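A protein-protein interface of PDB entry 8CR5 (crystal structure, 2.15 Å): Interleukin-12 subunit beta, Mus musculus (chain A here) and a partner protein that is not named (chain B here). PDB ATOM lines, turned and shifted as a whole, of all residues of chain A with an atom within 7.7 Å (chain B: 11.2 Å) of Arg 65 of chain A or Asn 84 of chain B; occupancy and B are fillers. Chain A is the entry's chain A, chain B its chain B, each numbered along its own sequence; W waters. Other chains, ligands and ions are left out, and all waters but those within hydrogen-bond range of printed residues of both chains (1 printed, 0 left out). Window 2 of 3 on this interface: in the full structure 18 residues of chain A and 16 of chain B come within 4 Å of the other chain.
The backbone carbonyl oxygen (O) of Gln 64 of chain A sits at hydrogen-bond distance from the guanidinium group (NH2) of Arg 92 of chain B (3.5 Å).
The guanidinium group (NH2) of Arg 65 of chain A sits close to the side-chain amide nitrogen (ND2) of Asn 84 of chain B, at 3.1 Å.
O of Ala 85 of chain A sits at hydrogen-bond distance from NE2 of Gln 64 of chain A.
N of Arg 92 of chain B sits at hydrogen-bond distance from O of Phe 80 of chain B (2.8 Å).
Arg 65 of chain A touches Arg 92 of chain B (CG to NH1, 3.6 Å).
Thr 76 of chain A touches His 85 of chain B (O to CE1, 3.6 Å).
His 85 of chain B touches Thr 78 of chain A (NE2 to OG1, 3.6 Å).
Leu 83 of chain A touches Pro 82 of chain B.
Arg 65 of chain A touches just these residues of chain B: Asn 84 and Arg 92.
No residue of chain B comes within 4 Å of Ser 62 of chain A.
Of the printed residues of chain B, Gln 64 of chain A touches Arg 92 (3.5 Å).
No residue of chain B comes within 4 Å of His 66 of chain A.
No residue of chain B comes within 4 Å of Gly 67 of chain A.
Thr 78 of chain A touches just one residue of chain B: His 85 (3.6 Å).
Printed residues of chain A within 4 Å of Arg 92 of chain B: Gln 64 (3.5 Å) and Arg 65 (3.6 Å).
Of the printed residues of chain A, Pro 82 of chain B touches Leu 83.
The nearest printed residue of chain A that does not touch Arg 92 of chain B is Leu 83 of chain A (4.4 Å).
Of the 19 printed residues of chain A, 5 touch a printed residue of chain B.
Hydrophobic or aromatic side chains of chain A within 4 Å of the printed part of chain B: Leu 83.
Hydrophobic or aromatic side chains of chain B within 4 Å of the printed part of chain A: Pro 82 and His 85.
Among the printed residues, 6 pairs touch across the chains.
Water W1 lies within hydrogen-bond range of OD1 of Asp 84 of chain A (2.9 Å) and O of Pro 83 of chain B (3.3 Å).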
ATOM      1  N   THR A  61      18.324  -8.478  -7.061  1.00  0.00           N
ATOM      2  CA  THR A  61      17.029  -7.830  -6.923  1.00  0.00           C
ATOM      3  C   THR A  61      16.849  -6.821  -8.048  1.00  0.00           C
ATOM      4  O   THR A  61      17.794  -6.461  -8.754  1.00  0.00           O
ATOM      5  CB  THR A  61      16.879  -7.134  -5.561  1.00  0.00           C
ATOM      6  OG1 THR A  61      17.950  -6.198  -5.376  1.00  0.00           O
ATOM      7  CG2 THR A  61      16.896  -8.153  -4.429  1.00  0.00           C
ATOM      8  N   SER A  62      15.609  -6.367  -8.209  1.00  0.00           N
ATOM      9  CA  SER A  62      15.256  -5.377  -9.214  1.00  0.00           C
ATOM     10  C   SER A  62      14.267  -4.398  -8.605  1.00  0.00           C
ATOM     11  O   SER A  62      13.389  -4.794  -7.833  1.00  0.00           O
ATOM     12  CB  SER A  62      14.655  -6.040 -10.463  1.00  0.00           C
ATOM     13  OG  SER A  62      14.269  -5.072 -11.423  1.00  0.00           O
ATOM     14  N   ASP A  63      14.409  -3.122  -8.952  1.00  0.00           N
ATOM     15  CA  ASP A  63      13.546  -2.093  -8.373  1.00  0.00           C
ATOM     16  C   ASP A  63      12.129  -2.117  -8.930  1.00  0.00           C
ATOM     17  O   ASP A  63      11.347  -1.206  -8.627  1.00  0.00           O
ATOM     18  CB  ASP A  63      14.165  -0.711  -8.580  1.00  0.00           C
ATOM     19  CG  ASP A  63      14.418  -0.397 -10.041  1.00  0.00           C
ATOM     20  OD1 ASP A  63      14.481  -1.345 -10.853  1.00  0.00           O
ATOM     21  OD2 ASP A  63      14.552   0.798 -10.376  1.00  0.00           O
ATOM     22  N   GLN A  64      11.776  -3.121  -9.730  1.00  0.00           N
ATOM     23  CA  GLN A  64      10.427  -3.263 -10.252  1.00  0.00           C
ATOM     24  C   GLN A  64       9.814  -4.617  -9.929  1.00  0.00           C
ATOM     25  O   GLN A  64       8.650  -4.852 -10.270  1.00  0.00           O
ATOM     26  CB  GLN A  64      10.416  -3.038 -11.766  1.00  0.00           C
ATOM     27  CG  GLN A  64      10.918  -1.668 -12.162  1.00  0.00           C
ATOM     28  CD  GLN A  64      10.563  -1.317 -13.583  1.00  0.00           C
ATOM     29  OE1 GLN A  64       9.391  -1.136 -13.910  1.00  0.00           O
ATOM     30  NE2 GLN A  64      11.570  -1.213 -14.440  1.00  0.00           N
ATOM     31  N   ARG A  65      10.564  -5.509  -9.290  1.00  0.00           N
ATOM     32  CA  ARG A  65      10.060  -6.784  -8.816  1.00  0.00           C
ATOM     33  C   ARG A  65      10.250  -6.866  -7.307  1.00  0.00           C
ATOM     34  O   ARG A  65      11.053  -6.136  -6.720  1.00  0.00           O
ATOM     35  CB  ARG A  65      10.772  -7.960  -9.501  1.00  0.00           C
ATOM     36  CG  ARG A  65      10.340  -8.199 -10.939  1.00  0.00           C
ATOM     37  CD  ARG A  65      11.474  -8.793 -11.760  1.00  0.00           C
ATOM     38  NE  ARG A  65      11.447 -10.251 -11.750  1.00  0.00           N
ATOM     39  CZ  ARG A  65      12.216 -11.020 -12.510  1.00  0.00           C
ATOM     40  NH1 ARG A  65      13.088 -10.500 -13.360  1.00  0.00           N
ATOM     41  NH2 ARG A  65      12.107 -12.341 -12.415  1.00  0.00           N
ATOM     42  N   HIS A  66       9.496  -7.761  -6.680  1.00  0.00           N
ATOM     43  CA  HIS A  66       9.561  -7.974  -5.241  1.00  0.00           C
ATOM     44  C   HIS A  66      10.283  -9.282  -4.956  1.00  0.00           C
ATOM     45  O   HIS A  66       9.959 -10.316  -5.548  1.00  0.00           O
ATOM     46  CB  HIS A  66       8.160  -7.991  -4.624  1.00  0.00           C
ATOM     47  CG  HIS A  66       7.483  -6.655  -4.628  1.00  0.00           C
ATOM     48  N   GLY A  67      11.263  -9.230  -4.056  1.00  0.00           N
ATOM     49  CA  GLY A  67      12.006 -10.412  -3.671  1.00  0.00           C
ATOM     50  C   GLY A  67      13.195 -10.688  -4.568  1.00  0.00           C
ATOM     51  O   GLY A  67      13.457 -10.004  -5.563  1.00  0.00           O
ATOM     52  N   VAL A  68      13.937 -11.731  -4.194  1.00  0.00           N
ATOM     53  CA  VAL A  68      15.112 -12.135  -4.955  1.00  0.00           C
ATOM     54  C   VAL A  68      14.673 -12.721  -6.290  1.00  0.00           C
ATOM     55  O   VAL A  68      13.754 -13.547  -6.352  1.00  0.00           O
ATOM     56  CB  VAL A  68      15.953 -13.138  -4.150  1.00  0.00           C
ATOM     57  CG1 VAL A  68      16.969 -13.832  -5.045  1.00  0.00           C
ATOM     58  CG2 VAL A  68      16.651 -12.435  -2.994  1.00  0.00           C
ATOM     59  N   ILE A  69      15.329 -12.290  -7.367  1.00  0.00           N
ATOM     60  CA  ILE A  69      14.991 -12.708  -8.722  1.00  0.00           C
ATOM     61  C   ILE A  69      16.027 -13.641  -9.320  1.00  0.00           C
ATOM     62  O   ILE A  69      15.868 -14.067 -10.474  1.00  0.00           O
ATOM     63  CB  ILE A  69      14.783 -11.491  -9.641  1.00  0.00           C
ATOM     64  CG1 ILE A  69      16.121 -10.793  -9.896  1.00  0.00           C
ATOM     65  CG2 ILE A  69      13.781 -10.526  -9.027  1.00  0.00           C
ATOM     66  CD1 ILE A  69      16.037  -9.640 -10.869  1.00  0.00           C
ATOM     67  N   GLY A  70      17.084 -13.971  -8.584  1.00  0.00           N
ATOM     68  CA  GLY A  70      18.129 -14.835  -9.099  1.00  0.00           C
ATOM     69  C   GLY A  70      19.335 -14.892  -8.186  1.00  0.00           C
ATOM     70  O   GLY A  70      19.487 -14.051  -7.296  1.00  0.00           O
ATOM     71  N   LEU A  75      23.641 -12.801 -13.661  1.00  0.00           N
ATOM     72  CA  LEU A  75      22.195 -12.933 -13.801  1.00  0.00           C
ATOM     73  C   LEU A  75      21.818 -12.738 -15.262  1.00  0.00           C
ATOM     74  O   LEU A  75      22.112 -11.691 -15.847  1.00  0.00           O
ATOM     75  CB  LEU A  75      21.464 -11.919 -12.922  1.00  0.00           C
ATOM     76  CG  LEU A  75      19.977 -11.759 -13.238  1.00  0.00           C
ATOM     77  CD1 LEU A  75      19.197 -12.972 -12.751  1.00  0.00           C
ATOM     78  CD2 LEU A  75      19.422 -10.479 -12.639  1.00  0.00           C
ATOM     79  N   THR A  76      21.159 -13.736 -15.842  1.00  0.00           N
ATOM     80  CA  THR A  76      20.752 -13.704 -17.242  1.00  0.00           C
ATOM     81  C   THR A  76      19.262 -13.407 -17.324  1.00  0.00           C
ATOM     82  O   THR A  76      18.440 -14.163 -16.792  1.00  0.00           O
ATOM     83  CB  THR A  76      21.076 -15.027 -17.938  1.00  0.00           C
ATOM     84  OG1 THR A  76      22.496 -15.208 -17.983  1.00  0.00           O
ATOM     85  CG2 THR A  76      20.526 -15.031 -19.356  1.00  0.00           C
ATOM     86  N   ILE A  77      18.915 -12.308 -17.994  1.00  0.00           N
ATOM     87  CA  ILE A  77      17.535 -11.873 -18.141  1.00  0.00           C
ATOM     88  C   ILE A  77      17.265 -11.576 -19.609  1.00  0.00           C
ATOM     89  O   ILE A  77      18.173 -11.280 -20.389  1.00  0.00           O
ATOM     90  CB  ILE A  77      17.216 -10.631 -17.281  1.00  0.00           C
ATOM     91  CG1 ILE A  77      18.179  -9.491 -17.626  1.00  0.00           C
ATOM     92  CG2 ILE A  77      17.282 -10.970 -15.801  1.00  0.00           C
ATOM     93  CD1 ILE A  77      17.882  -8.199 -16.901  1.00  0.00           C
ATOM     94  N   THR A  78      15.991 -11.662 -19.977  1.00  0.00           N
ATOM     95  CA  THR A  78      15.523 -11.255 -21.293  1.00  0.00           C
ATOM     96  C   THR A  78      14.796  -9.926 -21.154  1.00  0.00           C
ATOM     97  O   THR A  78      13.892  -9.793 -20.323  1.00  0.00           O
ATOM     98  CB  THR A  78      14.600 -12.311 -21.902  1.00  0.00           C
ATOM     99  OG1 THR A  78      15.347 -13.503 -22.176  1.00  0.00           O
ATOM    100  CG2 THR A  78      13.989 -11.803 -23.195  1.00  0.00           C
ATOM    101  N   LEU A  83       9.220  -2.887 -17.955  1.00  0.00           N
ATOM    102  CA  LEU A  83       9.231  -3.592 -16.678  1.00  0.00           C
ATOM    103  C   LEU A  83      10.468  -4.464 -16.518  1.00  0.00           C
ATOM    104  O   LEU A  83      10.802  -4.843 -15.390  1.00  0.00           O
ATOM    105  CB  LEU A  83       7.956  -4.427 -16.515  1.00  0.00           C
ATOM    106  CG  LEU A  83       7.908  -5.848 -17.077  1.00  0.00           C
ATOM    107  CD1 LEU A  83       6.720  -6.595 -16.494  1.00  0.00           C
ATOM    108  CD2 LEU A  83       7.817  -5.817 -18.594  1.00  0.00           C
ATOM    109  N   ASP A  84      11.161  -4.777 -17.611  1.00  0.00           N
ATOM    110  CA  ASP A  84      12.426  -5.497 -17.567  1.00  0.00           C
ATOM    111  C   ASP A  84      13.625  -4.575 -17.388  1.00  0.00           C
ATOM    112  O   ASP A  84      14.750  -5.065 -17.246  1.00  0.00           O
ATOM    113  CB  ASP A  84      12.611  -6.324 -18.843  1.00  0.00           C
ATOM    114  CG  ASP A  84      11.358  -7.075 -19.241  1.00  0.00           C
ATOM    115  OD1 ASP A  84      10.567  -7.428 -18.342  1.00  0.00           O
ATOM    116  OD2 ASP A  84      11.159  -7.302 -20.454  1.00  0.00           O
ATOM    117  N   ALA A  85      13.415  -3.263 -17.396  1.00  0.00           N
ATOM    118  CA  ALA A  85      14.492  -2.297 -17.256  1.00  0.00           C
ATOM    119  C   ALA A  85      14.545  -1.770 -15.825  1.00  0.00           C
ATOM    120  O   ALA A  85      13.768  -2.169 -14.955  1.00  0.00           O
ATOM    121  CB  ALA A  85      14.316  -1.156 -18.259  1.00  0.00           C
ATOM    122  N   GLN A  87      16.990  -0.515 -12.315  1.00  0.00           N
ATOM    123  CA  GLN A  87      18.191  -0.794 -11.540  1.00  0.00           C
ATOM    124  C   GLN A  87      18.180  -2.240 -11.063  1.00  0.00           C
ATOM    125  O   GLN A  87      17.215  -2.688 -10.435  1.00  0.00           O
ATOM    126  CB  GLN A  87      18.296   0.157 -10.349  1.00  0.00           C
ATOM    127  CG  GLN A  87      18.506   1.607 -10.746  1.00  0.00           C
ATOM    128  CD  GLN A  87      19.963   1.931 -11.017  1.00  0.00           C
ATOM    129  OE1 GLN A  87      20.833   1.068 -10.910  1.00  0.00           O
ATOM    130  NE2 GLN A  87      20.233   3.180 -11.375  1.00  0.00           N
ATOM    131  N   TYR A  88      19.250  -2.965 -11.373  1.00  0.00           N
ATOM    132  CA  TYR A  88      19.454  -4.325 -10.896  1.00  0.00           C
ATOM    133  C   TYR A  88      20.589  -4.317  -9.884  1.00  0.00           C
ATOM    134  O   TYR A  88      21.671  -3.792 -10.165  1.00  0.00           O
ATOM    135  CB  TYR A  88      19.770  -5.275 -12.053  1.00  0.00           C
ATOM    136  CG  TYR A  88      18.575  -5.608 -12.917  1.00  0.00           C
ATOM    137  CD1 TYR A  88      18.155  -4.743 -13.920  1.00  0.00           C
ATOM    138  CD2 TYR A  88      17.863  -6.788 -12.728  1.00  0.00           C
ATOM    139  CE1 TYR A  88      17.062  -5.042 -14.713  1.00  0.00           C
ATOM    140  CE2 TYR A  88      16.768  -7.096 -13.516  1.00  0.00           C
ATOM    141  CZ  TYR A  88      16.372  -6.218 -14.505  1.00  0.00           C
ATOM    142  OH  TYR A  88      15.284  -6.520 -15.292  1.00  0.00           O
ATOM    143  N   PHE B  80      -1.465  -9.793 -15.166  1.00  0.00           N
ATOM    144  CA  PHE B  80      -0.725 -10.252 -16.334  1.00  0.00           C
ATOM    145  C   PHE B  80       0.353 -11.232 -15.893  1.00  0.00           C
ATOM    146  O   PHE B  80       0.718 -11.297 -14.717  1.00  0.00           O
ATOM    147  CB  PHE B  80      -0.097  -9.077 -17.088  1.00  0.00           C
ATOM    148  CG  PHE B  80       0.780  -8.209 -16.229  1.00  0.00           C
ATOM    149  CD1 PHE B  80       2.127  -8.491 -16.080  1.00  0.00           C
ATOM    150  CD2 PHE B  80       0.254  -7.115 -15.563  1.00  0.00           C
ATOM    151  CE1 PHE B  80       2.933  -7.697 -15.287  1.00  0.00           C
ATOM    152  CE2 PHE B  80       1.055  -6.318 -14.769  1.00  0.00           C
ATOM    153  CZ  PHE B  80       2.396  -6.609 -14.632  1.00  0.00           C
ATOM    154  N   VAL B  81       0.865 -11.981 -16.862  1.00  0.00           N
ATOM    155  CA  VAL B  81       1.947 -12.939 -16.669  1.00  0.00           C
ATOM    156  C   VAL B  81       3.171 -12.410 -17.415  1.00  0.00           C
ATOM    157  O   VAL B  81       3.189 -12.415 -18.655  1.00  0.00           O
ATOM    158  CB  VAL B  81       1.555 -14.338 -17.158  1.00  0.00           C
ATOM    159  CG1 VAL B  81       2.662 -15.333 -16.860  1.00  0.00           C
ATOM    160  CG2 VAL B  81       0.246 -14.776 -16.514  1.00  0.00           C
ATOM    161  N   PRO B  82       4.204 -11.945 -16.718  1.00  0.00           N
ATOM    162  CA  PRO B  82       5.352 -11.334 -17.397  1.00  0.00           C
ATOM    163  C   PRO B  82       6.286 -12.390 -17.959  1.00  0.00           C
ATOM    164  O   PRO B  82       6.602 -13.377 -17.277  1.00  0.00           O
ATOM    165  CB  PRO B  82       6.036 -10.529 -16.278  1.00  0.00           C
ATOM    166  CG  PRO B  82       5.048 -10.510 -15.133  1.00  0.00           C
ATOM    167  CD  PRO B  82       4.301 -11.793 -15.259  1.00  0.00           C
ATOM    168  N   PRO B  83       6.743 -12.221 -19.200  1.00  0.00           N
ATOM    169  CA  PRO B  83       7.771 -13.122 -19.745  1.00  0.00           C
ATOM    170  C   PRO B  83       9.019 -13.113 -18.876  1.00  0.00           C
ATOM    171  O   PRO B  83       9.609 -12.061 -18.616  1.00  0.00           O
ATOM    172  CB  PRO B  83       8.039 -12.542 -21.138  1.00  0.00           C
ATOM    173  CG  PRO B  83       6.749 -11.884 -21.507  1.00  0.00           C
ATOM    174  CD  PRO B  83       6.233 -11.290 -20.222  1.00  0.00           C
ATOM    175  N   ASN B  84       9.421 -14.296 -18.429  1.00  0.00           N
ATOM    176  CA  ASN B  84      10.483 -14.421 -17.438  1.00  0.00           C
ATOM    177  C   ASN B  84      11.231 -15.725 -17.691  1.00  0.00           C
ATOM    178  O   ASN B  84      11.144 -16.309 -18.777  1.00  0.00           O
ATOM    179  CB  ASN B  84       9.891 -14.354 -16.019  1.00  0.00           C
ATOM    180  CG  ASN B  84      10.349 -13.132 -15.253  1.00  0.00           C
ATOM    181  OD1 ASN B  84      11.332 -12.488 -15.617  1.00  0.00           O
ATOM    182  ND2 ASN B  84       9.637 -12.809 -14.179  1.00  0.00           N
ATOM    183  N   HIS B  85      11.976 -16.179 -16.681  1.00  0.00           N
ATOM    184  CA  HIS B  85      12.618 -17.487 -16.686  1.00  0.00           C
ATOM    185  C   HIS B  85      11.975 -18.436 -15.680  1.00  0.00           C
ATOM    186  O   HIS B  85      12.567 -19.463 -15.332  1.00  0.00           O
ATOM    187  CB  HIS B  85      14.116 -17.350 -16.404  1.00  0.00           C
ATOM    188  CG  HIS B  85      14.883 -16.683 -17.504  1.00  0.00           C
ATOM    189  ND1 HIS B  85      16.126 -17.117 -17.910  1.00  0.00           N
ATOM    190  CD2 HIS B  85      14.586 -15.612 -18.277  1.00  0.00           C
ATOM    191  CE1 HIS B  85      16.561 -16.343 -18.890  1.00  0.00           C
ATOM    192  NE2 HIS B  85      15.645 -15.422 -19.132  1.00  0.00           N
ATOM    193  N   THR B  86      10.778 -18.105 -15.202  1.00  0.00           N
ATOM    194  CA  THR B  86      10.055 -18.927 -14.241  1.00  0.00           C
ATOM    195  C   THR B  86       8.984 -19.740 -14.956  1.00  0.00           C
ATOM    196  O   THR B  86       8.252 -19.217 -15.801  1.00  0.00           O
ATOM    197  CB  THR B  86       9.411 -18.065 -13.153  1.00  0.00           C
ATOM    198  OG1 THR B  86       8.323 -17.318 -13.712  1.00  0.00           O
ATOM    199  CG2 THR B  86      10.430 -17.099 -12.562  1.00  0.00           C
ATOM    200  N   HIS B  87       8.898 -21.027 -14.612  1.00  0.00           N
ATOM    201  CA  HIS B  87       7.912 -21.902 -15.234  1.00  0.00           C
ATOM    202  C   HIS B  87       6.545 -21.783 -14.574  1.00  0.00           C
ATOM    203  O   HIS B  87       5.524 -21.998 -15.237  1.00  0.00           O
ATOM    204  CB  HIS B  87       8.392 -23.354 -15.192  1.00  0.00           C
ATOM    205  N   THR B  88       6.502 -21.462 -13.283  1.00  0.00           N
ATOM    206  CA  THR B  88       5.233 -21.151 -12.642  1.00  0.00           C
ATOM    207  C   THR B  88       4.672 -19.860 -13.224  1.00  0.00           C
ATOM    208  O   THR B  88       5.423 -18.952 -13.588  1.00  0.00           O
ATOM    209  CB  THR B  88       5.409 -21.019 -11.129  1.00  0.00           C
ATOM    210  OG1 THR B  88       6.597 -20.268 -10.846  1.00  0.00           O
ATOM    211  CG2 THR B  88       5.515 -22.393 -10.482  1.00  0.00           C
ATOM    212  N   GLY B  89       3.342 -19.791 -13.319  1.00  0.00           N
ATOM    213  CA  GLY B  89       2.708 -18.641 -13.948  1.00  0.00           C
ATOM    214  C   GLY B  89       3.149 -17.322 -13.349  1.00  0.00           C
ATOM    215  O   GLY B  89       3.614 -16.428 -14.059  1.00  0.00           O
ATOM    216  N   GLN B  90       3.022 -17.191 -12.028  1.00  0.00           N
ATOM    217  CA  GLN B  90       3.437 -15.991 -11.300  1.00  0.00           C
ATOM    218  C   GLN B  90       2.715 -14.752 -11.832  1.00  0.00           C
ATOM    219  O   GLN B  90       3.323 -13.810 -12.344  1.00  0.00           O
ATOM    220  CB  GLN B  90       4.958 -15.809 -11.358  1.00  0.00           C
ATOM    221  CG  GLN B  90       5.726 -16.630 -10.339  1.00  0.00           C
ATOM    222  CD  GLN B  90       7.103 -16.061 -10.065  1.00  0.00           C
ATOM    223  OE1 GLN B  90       7.650 -15.318 -10.880  1.00  0.00           O
ATOM    224  NE2 GLN B  90       7.673 -16.406  -8.915  1.00  0.00           N
ATOM    225  N   GLU B  91       1.391 -14.776 -11.705  1.00  0.00           N
ATOM    226  CA  GLU B  91       0.570 -13.659 -12.150  1.00  0.00           C
ATOM    227  C   GLU B  91       0.818 -12.438 -11.272  1.00  0.00           C
ATOM    228  O   GLU B  91       0.860 -12.540 -10.042  1.00  0.00           O
ATOM    229  CB  GLU B  91      -0.905 -14.055 -12.117  1.00  0.00           C
ATOM    230  CG  GLU B  91      -1.879 -12.926 -12.388  1.00  0.00           C
ATOM    231  CD  GLU B  91      -3.274 -13.245 -11.890  1.00  0.00           C
ATOM    232  OE1 GLU B  91      -3.392 -13.909 -10.837  1.00  0.00           O
ATOM    233  OE2 GLU B  91      -4.252 -12.843 -12.552  1.00  0.00           O
ATOM    234  N   ARG B  92       0.994 -11.282 -11.906  1.00  0.00           N
ATOM    235  CA  ARG B  92       1.245 -10.025 -11.215  1.00  0.00           C
ATOM    236  C   ARG B  92       0.083  -9.075 -11.463  1.00  0.00           C
ATOM    237  O   ARG B  92      -0.421  -8.978 -12.586  1.00  0.00           O
ATOM    238  CB  ARG B  92       2.558  -9.390 -11.686  1.00  0.00           C
ATOM    239  CG  ARG B  92       3.729 -10.361 -11.730  1.00  0.00           C
ATOM    240  CD  ARG B  92       4.930  -9.839 -10.961  1.00  0.00           C
ATOM    241  NE  ARG B  92       5.179  -8.428 -11.230  1.00  0.00           N
ATOM    242  CZ  ARG B  92       6.207  -7.965 -11.926  1.00  0.00           C
ATOM    243  NH1 ARG B  92       7.111  -8.779 -12.449  1.00  0.00           N
ATOM    244  NH2 ARG B  92       6.334  -6.653 -12.104  1.00  0.00           N
ATOM    245  N   CYS B  93      -0.337  -8.367 -10.415  1.00  0.00           N
ATOM    246  CA  CYS B  93      -1.536  -7.545 -10.474  1.00  0.00           C
ATOM    247  C   CYS B  93      -1.247  -6.128  -9.998  1.00  0.00           C
ATOM    248  O   CYS B  93      -0.460  -5.918  -9.070  1.00  0.00           O
ATOM    249  CB  CYS B  93      -2.664  -8.159  -9.632  1.00  0.00           C
ATOM    250  SG  CYS B  93      -3.280  -9.738 -10.274  1.00  0.00           S
ATOM    251  N   ARG B  94      -1.890  -5.161 -10.652  1.00  0.00           N
ATOM    252  CA  ARG B  94      -1.843  -3.755 -10.277  1.00  0.00           C
ATOM    253  C   ARG B  94      -3.264  -3.210 -10.275  1.00  0.00           C
ATOM    254  O   ARG B  94      -4.171  -3.798 -10.869  1.00  0.00           O
ATOM    255  CB  ARG B  94      -0.974  -2.929 -11.240  1.00  0.00           C
ATOM    256  CG  ARG B  94       0.316  -3.601 -11.678  1.00  0.00           C
ATOM    257  CD  ARG B  94       1.435  -3.307 -10.700  1.00  0.00           C
ATOM    258  NE  ARG B  94       2.584  -4.181 -10.907  1.00  0.00           N
ATOM    259  CZ  ARG B  94       2.865  -5.233 -10.151  1.00  0.00           C
ATOM    260  NH1 ARG B  94       2.083  -5.591  -9.146  1.00  0.00           N
ATOM    261  NH2 ARG B  94       3.957  -5.944 -10.412  1.00  0.00           N
ATOM    262  N   ASP B 110       4.778   2.952 -16.247  1.00  0.00           N
ATOM    263  CA  ASP B 110       4.062   2.770 -14.990  1.00  0.00           C
ATOM    264  C   ASP B 110       4.113   1.343 -14.470  1.00  0.00           C
ATOM    265  O   ASP B 110       3.669   1.101 -13.345  1.00  0.00           O
ATOM    266  CB  ASP B 110       2.595   3.185 -15.127  1.00  0.00           C
ATOM    267  CG  ASP B 110       2.361   4.617 -14.707  1.00  0.00           C
ATOM    268  OD1 ASP B 110       3.003   5.039 -13.727  1.00  0.00           O
ATOM    269  OD2 ASP B 110       1.552   5.307 -15.359  1.00  0.00           O
ATOM    270  N   GLY B 111       4.622   0.396 -15.253  1.00  0.00           N
ATOM    271  CA  GLY B 111       4.781  -0.970 -14.796  1.00  0.00           C
ATOM    272  C   GLY B 111       3.848  -1.982 -15.425  1.00  0.00           C
ATOM    273  O   GLY B 111       3.902  -3.159 -15.048  1.00  0.00           O
ATOM    274  N   ILE B 112       3.002  -1.578 -16.361  1.00  0.00           N
ATOM    275  CA  ILE B 112       2.077  -2.481 -17.041  1.00  0.00           C
ATOM    276  C   ILE B 112       2.634  -2.776 -18.429  1.00  0.00           C
ATOM    277  O   ILE B 112       2.964  -1.833 -19.160  1.00  0.00           O
ATOM    278  CB  ILE B 112       0.664  -1.878 -17.139  1.00  0.00           C
ATOM    279  CG1 ILE B 112      -0.031  -1.912 -15.776  1.00  0.00           C
ATOM    280  CG2 ILE B 112      -0.165  -2.626 -18.171  1.00  0.00           C
ATOM    281  CD1 ILE B 112      -1.448  -1.379 -15.802  1.00  0.00           C
ATOM    282  N   PRO B 113       2.755  -4.043 -18.824  1.00  0.00           N
ATOM    283  CA  PRO B 113       3.298  -4.347 -20.154  1.00  0.00           C
ATOM    284  C   PRO B 113       2.355  -3.893 -21.255  1.00  0.00           C
ATOM    285  O   PRO B 113       1.133  -4.008 -21.139  1.00  0.00           O
ATOM    286  CB  PRO B 113       3.445  -5.874 -20.142  1.00  0.00           C
ATOM    287  CG  PRO B 113       3.325  -6.281 -18.699  1.00  0.00           C
ATOM    288  CD  PRO B 113       2.439  -5.261 -18.063  1.00  0.00           C
ATOM    289  N   SER B 116       2.648  -7.322 -24.419  1.00  0.00           N
ATOM    290  CA  SER B 116       2.218  -8.676 -24.102  1.00  0.00           C
ATOM    291  C   SER B 116       0.787  -8.639 -23.586  1.00  0.00           C
ATOM    292  O   SER B 116       0.250  -7.581 -23.245  1.00  0.00           O
ATOM    293  CB  SER B 116       3.148  -9.346 -23.083  1.00  0.00           C
ATOM    294  OG  SER B 116       3.658  -8.406 -22.154  1.00  0.00           O
HETATM  295  O   HOH W   1       8.292  -9.113 -19.057  1.00  0.00           O
